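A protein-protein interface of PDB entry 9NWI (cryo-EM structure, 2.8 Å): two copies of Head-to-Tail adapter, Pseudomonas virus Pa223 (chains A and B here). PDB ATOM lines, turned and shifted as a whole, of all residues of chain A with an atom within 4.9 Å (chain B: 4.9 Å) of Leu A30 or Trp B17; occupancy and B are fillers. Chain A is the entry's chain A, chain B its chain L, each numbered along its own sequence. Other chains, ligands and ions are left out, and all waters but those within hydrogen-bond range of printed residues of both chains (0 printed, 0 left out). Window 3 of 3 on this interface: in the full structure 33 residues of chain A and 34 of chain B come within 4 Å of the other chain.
CG2 of Thr B3 touches CD1 of Leu A30 (3.6 Å). NE1 of Trp B17 touches CD2 of Leu A30, 3.6 Å away. Phe A31 touches Trp B17. CG2 of Thr B3 touches OD1 of Asn A34 (3.98 Å). CH2 of Trp B17 touches OE1 of Gln A162, at 3.9 Å. CE1 of Tyr A166 touches O of Gln B16, 3.9 Å away. SD of Met A168 touches OH of Tyr B164, 3.9 Å away.
No position is printed for both chains. Of the 7 pairs that touch across the chains among the printed residues, none has its exchanged pair printed and touching as well.
Of chain B, only Thr B3 (3.6 Å) and Trp B17 (3.6 Å) come within 4 Å of Leu A30. Printed residues of chain B within 4 Å of Phe A31: Trp B17 (3.5 Å). Printed residues of chain B within 4 Å of Asn A34: Thr B3 (3.98 Å). Of the printed residues of chain B, Tyr A166 touches Gln B16 (3.9 Å). Printed residues of chain A within 4 Å of Gln B16: Tyr A166 (3.9 Å). Of the printed residues of chain A, Trp B17 touches Leu A30, Phe A31 and Gln A162. The nearest residue of chain B that does not touch Leu A30 is Ile B4 (4.2 Å). The nearest printed residue of chain A that does not touch Trp B17 is Tyr A166 (4.01 Å). The nearest printed residue of chain B that does not touch Asn A34 is Leu B156 (4.5 Å).
The side-chain amide oxygen (OE1) of Gln A162 is in hydrogen-bond range of the side-chain amide nitrogen (ND2) of Asn A34.
Hydrophobic or aromatic side chains of chain B that line the printed part of chain A: Trp B17 and Tyr B164.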
ATOM      1  N   GLU A  26     -23.538  30.450 -16.477  1.00  0.00           N
ATOM      2  CA  GLU A  26     -22.810  29.499 -15.646  1.00  0.00           C
ATOM      3  C   GLU A  26     -23.691  28.943 -14.536  1.00  0.00           C
ATOM      4  O   GLU A  26     -23.646  27.743 -14.240  1.00  0.00           O
ATOM      5  CB  GLU A  26     -21.565  30.162 -15.062  1.00  0.00           C
ATOM      6  CG  GLU A  26     -20.396  30.234 -16.026  1.00  0.00           C
ATOM      7  CD  GLU A  26     -20.665  31.149 -17.204  1.00  0.00           C
ATOM      8  OE1 GLU A  26     -21.453  32.104 -17.047  1.00  0.00           O
ATOM      9  OE2 GLU A  26     -20.091  30.911 -18.286  1.00  0.00           O
ATOM     10  N   LEU A  27     -24.499  29.799 -13.910  1.00  0.00           N
ATOM     11  CA  LEU A  27     -25.390  29.328 -12.856  1.00  0.00           C
ATOM     12  C   LEU A  27     -26.429  28.358 -13.402  1.00  0.00           C
ATOM     13  O   LEU A  27     -26.743  27.348 -12.762  1.00  0.00           O
ATOM     14  CB  LEU A  27     -26.067  30.516 -12.177  1.00  0.00           C
ATOM     15  CG  LEU A  27     -25.163  31.386 -11.306  1.00  0.00           C
ATOM     16  CD1 LEU A  27     -25.993  32.219 -10.351  1.00  0.00           C
ATOM     17  CD2 LEU A  27     -24.171  30.531 -10.545  1.00  0.00           C
ATOM     18  N   LEU A  28     -26.981  28.651 -14.581  1.00  0.00           N
ATOM     19  CA  LEU A  28     -27.951  27.743 -15.182  1.00  0.00           C
ATOM     20  C   LEU A  28     -27.316  26.400 -15.513  1.00  0.00           C
ATOM     21  O   LEU A  28     -27.922  25.345 -15.289  1.00  0.00           O
ATOM     22  CB  LEU A  28     -28.555  28.377 -16.432  1.00  0.00           C
ATOM     23  CG  LEU A  28     -29.540  29.514 -16.172  1.00  0.00           C
ATOM     24  CD1 LEU A  28     -29.868  30.240 -17.463  1.00  0.00           C
ATOM     25  CD2 LEU A  28     -30.799  28.982 -15.522  1.00  0.00           C
ATOM     26  N   MET A  29     -26.093  26.419 -16.046  1.00  0.00           N
ATOM     27  CA  MET A  29     -25.399  25.167 -16.326  1.00  0.00           C
ATOM     28  C   MET A  29     -25.139  24.387 -15.045  1.00  0.00           C
ATOM     29  O   MET A  29     -25.269  23.158 -15.021  1.00  0.00           O
ATOM     30  CB  MET A  29     -24.092  25.444 -17.064  1.00  0.00           C
ATOM     31  CG  MET A  29     -24.282  25.794 -18.526  1.00  0.00           C
ATOM     32  SD  MET A  29     -25.638  24.874 -19.270  1.00  0.00           S
ATOM     33  CE  MET A  29     -26.626  26.207 -19.941  1.00  0.00           C
ATOM     34  N   LEU A  30     -24.775  25.085 -13.969  1.00  0.00           N
ATOM     35  CA  LEU A  30     -24.563  24.418 -12.689  1.00  0.00           C
ATOM     36  C   LEU A  30     -25.846  23.774 -12.181  1.00  0.00           C
ATOM     37  O   LEU A  30     -25.828  22.640 -11.690  1.00  0.00           O
ATOM     38  CB  LEU A  30     -24.022  25.417 -11.670  1.00  0.00           C
ATOM     39  CG  LEU A  30     -23.814  24.914 -10.244  1.00  0.00           C
ATOM     40  CD1 LEU A  30     -22.647  23.957 -10.191  1.00  0.00           C
ATOM     41  CD2 LEU A  30     -23.588  26.080  -9.303  1.00  0.00           C
ATOM     42  N   PHE A  31     -26.972  24.484 -12.289  1.00  0.00           N
ATOM     43  CA  PHE A  31     -28.244  23.922 -11.846  1.00  0.00           C
ATOM     44  C   PHE A  31     -28.616  22.690 -12.662  1.00  0.00           C
ATOM     45  O   PHE A  31     -29.060  21.674 -12.109  1.00  0.00           O
ATOM     46  CB  PHE A  31     -29.350  24.971 -11.945  1.00  0.00           C
ATOM     47  CG  PHE A  31     -29.095  26.207 -11.136  1.00  0.00           C
ATOM     48  CD1 PHE A  31     -28.340  26.154  -9.980  1.00  0.00           C
ATOM     49  CD2 PHE A  31     -29.617  27.426 -11.531  1.00  0.00           C
ATOM     50  CE1 PHE A  31     -28.107  27.292  -9.237  1.00  0.00           C
ATOM     51  CE2 PHE A  31     -29.387  28.565 -10.791  1.00  0.00           C
ATOM     52  CZ  PHE A  31     -28.632  28.498  -9.644  1.00  0.00           C
ATOM     53  N   ILE A  32     -28.441  22.764 -13.981  1.00  0.00           N
ATOM     54  CA  ILE A  32     -28.768  21.629 -14.839  1.00  0.00           C
ATOM     55  C   ILE A  32     -27.878  20.438 -14.507  1.00  0.00           C
ATOM     56  O   ILE A  32     -28.345  19.294 -14.438  1.00  0.00           O
ATOM     57  CB  ILE A  32     -28.656  22.033 -16.318  1.00  0.00           C
ATOM     58  CG1 ILE A  32     -29.749  23.039 -16.671  1.00  0.00           C
ATOM     59  CG2 ILE A  32     -28.752  20.817 -17.213  1.00  0.00           C
ATOM     60  CD1 ILE A  32     -29.507  23.770 -17.965  1.00  0.00           C
ATOM     61  N   GLY A  33     -26.586  20.687 -14.293  1.00  0.00           N
ATOM     62  CA  GLY A  33     -25.691  19.608 -13.918  1.00  0.00           C
ATOM     63  C   GLY A  33     -26.067  18.974 -12.595  1.00  0.00           C
ATOM     64  O   GLY A  33     -26.014  17.753 -12.446  1.00  0.00           O
ATOM     65  N   ASN A  34     -26.450  19.796 -11.614  1.00  0.00           N
ATOM     66  CA  ASN A  34     -26.874  19.252 -10.329  1.00  0.00           C
ATOM     67  C   ASN A  34     -28.106  18.374 -10.486  1.00  0.00           C
ATOM     68  O   ASN A  34     -28.190  17.291  -9.892  1.00  0.00           O
ATOM     69  CB  ASN A  34     -27.150  20.386  -9.345  1.00  0.00           C
ATOM     70  CG  ASN A  34     -25.940  20.740  -8.515  1.00  0.00           C
ATOM     71  OD1 ASN A  34     -24.984  19.972  -8.436  1.00  0.00           O
ATOM     72  ND2 ASN A  34     -25.974  21.908  -7.889  1.00  0.00           N
ATOM     73  N   GLN A 162     -33.481  24.207  -7.881  1.00  0.00           N
ATOM     74  CA  GLN A 162     -32.120  24.696  -7.695  1.00  0.00           C
ATOM     75  C   GLN A 162     -32.087  26.217  -7.627  1.00  0.00           C
ATOM     76  O   GLN A 162     -31.361  26.796  -6.810  1.00  0.00           O
ATOM     77  CB  GLN A 162     -31.222  24.191  -8.822  1.00  0.00           C
ATOM     78  CG  GLN A 162     -30.988  22.698  -8.794  1.00  0.00           C
ATOM     79  CD  GLN A 162     -30.046  22.284  -7.690  1.00  0.00           C
ATOM     80  OE1 GLN A 162     -28.883  22.678  -7.670  1.00  0.00           O
ATOM     81  NE2 GLN A 162     -30.546  21.484  -6.757  1.00  0.00           N
ATOM     82  N   LEU A 165     -33.303  27.334  -4.318  1.00  0.00           N
ATOM     83  CA  LEU A 165     -32.265  27.069  -3.329  1.00  0.00           C
ATOM     84  C   LEU A 165     -31.185  28.140  -3.377  1.00  0.00           C
ATOM     85  O   LEU A 165     -30.651  28.541  -2.338  1.00  0.00           O
ATOM     86  CB  LEU A 165     -31.654  25.690  -3.564  1.00  0.00           C
ATOM     87  CG  LEU A 165     -32.267  24.522  -2.796  1.00  0.00           C
ATOM     88  CD1 LEU A 165     -31.499  23.249  -3.084  1.00  0.00           C
ATOM     89  CD2 LEU A 165     -32.280  24.815  -1.312  1.00  0.00           C
ATOM     90  N   TYR A 166     -30.851  28.608  -4.580  1.00  0.00           N
ATOM     91  CA  TYR A 166     -29.789  29.596  -4.734  1.00  0.00           C
ATOM     92  C   TYR A 166     -30.157  30.924  -4.082  1.00  0.00           C
ATOM     93  O   TYR A 166     -29.305  31.581  -3.477  1.00  0.00           O
ATOM     94  CB  TYR A 166     -29.478  29.792  -6.215  1.00  0.00           C
ATOM     95  CG  TYR A 166     -28.574  30.960  -6.515  1.00  0.00           C
ATOM     96  CD1 TYR A 166     -27.205  30.865  -6.328  1.00  0.00           C
ATOM     97  CD2 TYR A 166     -29.087  32.154  -6.997  1.00  0.00           C
ATOM     98  CE1 TYR A 166     -26.374  31.927  -6.605  1.00  0.00           C
ATOM     99  CE2 TYR A 166     -28.263  33.220  -7.276  1.00  0.00           C
ATOM    100  CZ  TYR A 166     -26.908  33.100  -7.079  1.00  0.00           C
ATOM    101  OH  TYR A 166     -26.082  34.162  -7.356  1.00  0.00           O
ATOM    102  N   MET A 168     -31.761  31.549  -1.466  1.00  0.00           N
ATOM    103  CA  MET A 168     -32.010  31.397  -0.029  1.00  0.00           C
ATOM    104  C   MET A 168     -33.500  31.476   0.302  1.00  0.00           C
ATOM    105  O   MET A 168     -33.935  32.270   1.136  1.00  0.00           O
ATOM    106  CB  MET A 168     -31.208  32.414   0.792  1.00  0.00           C
ATOM    107  CG  MET A 168     -30.048  33.074   0.059  1.00  0.00           C
ATOM    108  SD  MET A 168     -28.846  33.833   1.164  1.00  0.00           S
ATOM    109  CE  MET A 168     -29.653  35.391   1.517  1.00  0.00           C
ATOM    110  N   THR B   3     -19.792  19.579 -13.951  1.00  0.00           N
ATOM    111  CA  THR B   3     -20.347  20.429 -12.903  1.00  0.00           C
ATOM    112  C   THR B   3     -19.237  21.208 -12.209  1.00  0.00           C
ATOM    113  O   THR B   3     -18.831  22.272 -12.685  1.00  0.00           O
ATOM    114  CB  THR B   3     -21.140  19.596 -11.894  1.00  0.00           C
ATOM    115  OG1 THR B   3     -21.921  18.619 -12.592  1.00  0.00           O
ATOM    116  CG2 THR B   3     -22.071  20.482 -11.093  1.00  0.00           C
ATOM    117  N   ILE B   4     -18.741  20.690 -11.090  1.00  0.00           N
ATOM    118  CA  ILE B   4     -17.616  21.275 -10.371  1.00  0.00           C
ATOM    119  C   ILE B   4     -16.405  20.379 -10.585  1.00  0.00           C
ATOM    120  O   ILE B   4     -16.460  19.177 -10.307  1.00  0.00           O
ATOM    121  CB  ILE B   4     -17.925  21.442  -8.876  1.00  0.00           C
ATOM    122  CG1 ILE B   4     -19.098  22.401  -8.684  1.00  0.00           C
ATOM    123  CG2 ILE B   4     -16.705  21.951  -8.136  1.00  0.00           C
ATOM    124  CD1 ILE B   4     -19.863  22.176  -7.407  1.00  0.00           C
ATOM    125  N   ALA B  13     -18.182  28.625  -6.039  1.00  0.00           N
ATOM    126  CA  ALA B  13     -19.595  28.302  -5.890  1.00  0.00           C
ATOM    127  C   ALA B  13     -20.071  28.561  -4.470  1.00  0.00           C
ATOM    128  O   ALA B  13     -21.179  29.065  -4.261  1.00  0.00           O
ATOM    129  CB  ALA B  13     -19.846  26.848  -6.284  1.00  0.00           C
ATOM    130  N   ALA B  14     -19.252  28.214  -3.476  1.00  0.00           N
ATOM    131  CA  ALA B  14     -19.623  28.485  -2.091  1.00  0.00           C
ATOM    132  C   ALA B  14     -19.754  29.980  -1.842  1.00  0.00           C
ATOM    133  O   ALA B  14     -20.704  30.428  -1.188  1.00  0.00           O
ATOM    134  CB  ALA B  14     -18.596  27.871  -1.144  1.00  0.00           C
ATOM    135  N   ILE B  15     -18.815  30.770  -2.365  1.00  0.00           N
ATOM    136  CA  ILE B  15     -18.886  32.218  -2.198  1.00  0.00           C
ATOM    137  C   ILE B  15     -20.155  32.764  -2.835  1.00  0.00           C
ATOM    138  O   ILE B  15     -20.854  33.598  -2.247  1.00  0.00           O
ATOM    139  CB  ILE B  15     -17.629  32.886  -2.784  1.00  0.00           C
ATOM    140  CG1 ILE B  15     -16.405  32.574  -1.926  1.00  0.00           C
ATOM    141  CG2 ILE B  15     -17.824  34.385  -2.889  1.00  0.00           C
ATOM    142  CD1 ILE B  15     -16.635  32.769  -0.453  1.00  0.00           C
ATOM    143  N   GLN B  16     -20.474  32.305  -4.045  1.00  0.00           N
ATOM    144  CA  GLN B  16     -21.651  32.814  -4.741  1.00  0.00           C
ATOM    145  C   GLN B  16     -22.940  32.421  -4.031  1.00  0.00           C
ATOM    146  O   GLN B  16     -23.849  33.245  -3.886  1.00  0.00           O
ATOM    147  CB  GLN B  16     -21.667  32.311  -6.182  1.00  0.00           C
ATOM    148  CG  GLN B  16     -20.503  32.793  -7.016  1.00  0.00           C
ATOM    149  CD  GLN B  16     -20.754  32.642  -8.498  1.00  0.00           C
ATOM    150  OE1 GLN B  16     -21.425  33.468  -9.111  1.00  0.00           O
ATOM    151  NE2 GLN B  16     -20.219  31.580  -9.083  1.00  0.00           N
ATOM    152  N   TRP B  17     -23.042  31.170  -3.582  1.00  0.00           N
ATOM    153  CA  TRP B  17     -24.286  30.704  -2.982  1.00  0.00           C
ATOM    154  C   TRP B  17     -24.499  31.312  -1.602  1.00  0.00           C
ATOM    155  O   TRP B  17     -25.604  31.762  -1.277  1.00  0.00           O
ATOM    156  CB  TRP B  17     -24.295  29.180  -2.905  1.00  0.00           C
ATOM    157  CG  TRP B  17     -24.569  28.516  -4.212  1.00  0.00           C
ATOM    158  CD1 TRP B  17     -23.933  28.742  -5.394  1.00  0.00           C
ATOM    159  CD2 TRP B  17     -25.554  27.514  -4.473  1.00  0.00           C
ATOM    160  NE1 TRP B  17     -24.459  27.941  -6.375  1.00  0.00           N
ATOM    161  CE2 TRP B  17     -25.458  27.178  -5.834  1.00  0.00           C
ATOM    162  CE3 TRP B  17     -26.509  26.868  -3.686  1.00  0.00           C
ATOM    163  CZ2 TRP B  17     -26.278  26.226  -6.426  1.00  0.00           C
ATOM    164  CZ3 TRP B  17     -27.322  25.923  -4.275  1.00  0.00           C
ATOM    165  CH2 TRP B  17     -27.202  25.611  -5.631  1.00  0.00           C
ATOM    166  N   SER B  18     -23.455  31.333  -0.774  1.00  0.00           N
ATOM    167  CA  SER B  18     -23.611  31.871   0.572  1.00  0.00           C
ATOM    168  C   SER B  18     -23.773  33.383   0.559  1.00  0.00           C
ATOM    169  O   SER B  18     -24.406  33.942   1.461  1.00  0.00           O
ATOM    170  CB  SER B  18     -22.416  31.478   1.436  1.00  0.00           C
ATOM    171  OG  SER B  18     -21.208  31.925   0.852  1.00  0.00           O
ATOM    172  N   ASP B  19     -23.222  34.051  -0.450  1.00  0.00           N
ATOM    173  CA  ASP B  19     -23.206  35.508  -0.547  1.00  0.00           C
ATOM    174  C   ASP B  19     -22.563  36.062   0.730  1.00  0.00           C
ATOM    175  O   ASP B  19     -23.206  36.583   1.638  1.00  0.00           O
ATOM    176  CB  ASP B  19     -24.631  36.021  -0.841  1.00  0.00           C
ATOM    177  CG  ASP B  19     -24.820  37.545  -0.670  1.00  0.00           C
ATOM    178  OD1 ASP B  19     -25.609  38.098  -1.464  1.00  0.00           O
ATOM    179  OD2 ASP B  19     -24.219  38.218   0.185  1.00  0.00           O
ATOM    180  N   LEU B 156     -20.565  20.627  -1.960  1.00  0.00           N
ATOM    181  CA  LEU B 156     -21.202  21.940  -1.940  1.00  0.00           C
ATOM    182  C   LEU B 156     -22.076  22.107  -0.702  1.00  0.00           C
ATOM    183  O   LEU B 156     -21.981  23.114   0.012  1.00  0.00           O
ATOM    184  CB  LEU B 156     -22.023  22.140  -3.212  1.00  0.00           C
ATOM    185  CG  LEU B 156     -22.559  23.550  -3.450  1.00  0.00           C
ATOM    186  CD1 LEU B 156     -21.432  24.558  -3.407  1.00  0.00           C
ATOM    187  CD2 LEU B 156     -23.288  23.619  -4.776  1.00  0.00           C
ATOM    188  N   LEU B 160     -21.525  24.600   2.534  1.00  0.00           N
ATOM    189  CA  LEU B 160     -22.554  25.566   2.910  1.00  0.00           C
ATOM    190  C   LEU B 160     -22.968  25.395   4.367  1.00  0.00           C
ATOM    191  O   LEU B 160     -23.154  26.385   5.091  1.00  0.00           O
ATOM    192  CB  LEU B 160     -23.763  25.429   1.989  1.00  0.00           C
ATOM    193  CG  LEU B 160     -23.621  26.130   0.639  1.00  0.00           C
ATOM    194  CD1 LEU B 160     -24.849  25.898  -0.216  1.00  0.00           C
ATOM    195  CD2 LEU B 160     -23.379  27.610   0.841  1.00  0.00           C
ATOM    196  N   TYR B 164     -22.609  28.255   7.331  1.00  0.00           N
ATOM    197  CA  TYR B 164     -23.690  28.744   8.177  1.00  0.00           C
ATOM    198  C   TYR B 164     -23.479  28.395   9.643  1.00  0.00           C
ATOM    199  O   TYR B 164     -24.006  29.093  10.513  1.00  0.00           O
ATOM    200  CB  TYR B 164     -25.030  28.214   7.680  1.00  0.00           C
ATOM    201  CG  TYR B 164     -25.547  29.011   6.512  1.00  0.00           C
ATOM    202  CD1 TYR B 164     -25.844  30.357   6.650  1.00  0.00           C
ATOM    203  CD2 TYR B 164     -25.710  28.429   5.268  1.00  0.00           C
ATOM    204  CE1 TYR B 164     -26.302  31.096   5.586  1.00  0.00           C
ATOM    205  CE2 TYR B 164     -26.170  29.161   4.197  1.00  0.00           C
ATOM    206  CZ  TYR B 164     -26.464  30.493   4.361  1.00  0.00           C
ATOM    207  OH  TYR B 164     -26.925  31.226   3.295  1.00  0.00           O
ATOM    208  N   TRP B 176     -29.077  22.659   5.570  1.00  0.00           N
ATOM    209  CA  TRP B 176     -28.000  22.173   4.717  1.00  0.00           C
ATOM    210  C   TRP B 176     -27.436  20.850   5.217  1.00  0.00           C
ATOM    211  O   TRP B 176     -27.033  20.008   4.407  1.00  0.00           O
ATOM    212  CB  TRP B 176     -26.904  23.228   4.609  1.00  0.00           C
ATOM    213  CG  TRP B 176     -27.322  24.404   3.787  1.00  0.00           C
ATOM    214  CD1 TRP B 176     -27.464  25.688   4.212  1.00  0.00           C
ATOM    215  CD2 TRP B 176     -27.669  24.400   2.399  1.00  0.00           C
ATOM    216  NE1 TRP B 176     -27.870  26.488   3.175  1.00  0.00           N
ATOM    217  CE2 TRP B 176     -28.005  25.720   2.049  1.00  0.00           C
ATOM    218  CE3 TRP B 176     -27.725  23.410   1.416  1.00  0.00           C
ATOM    219  CZ2 TRP B 176     -28.390  26.075   0.763  1.00  0.00           C
ATOM    220  CZ3 TRP B 176     -28.108  23.764   0.141  1.00  0.00           C
ATOM    221  CH2 TRP B 176     -28.435  25.084  -0.176  1.00  0.00           C
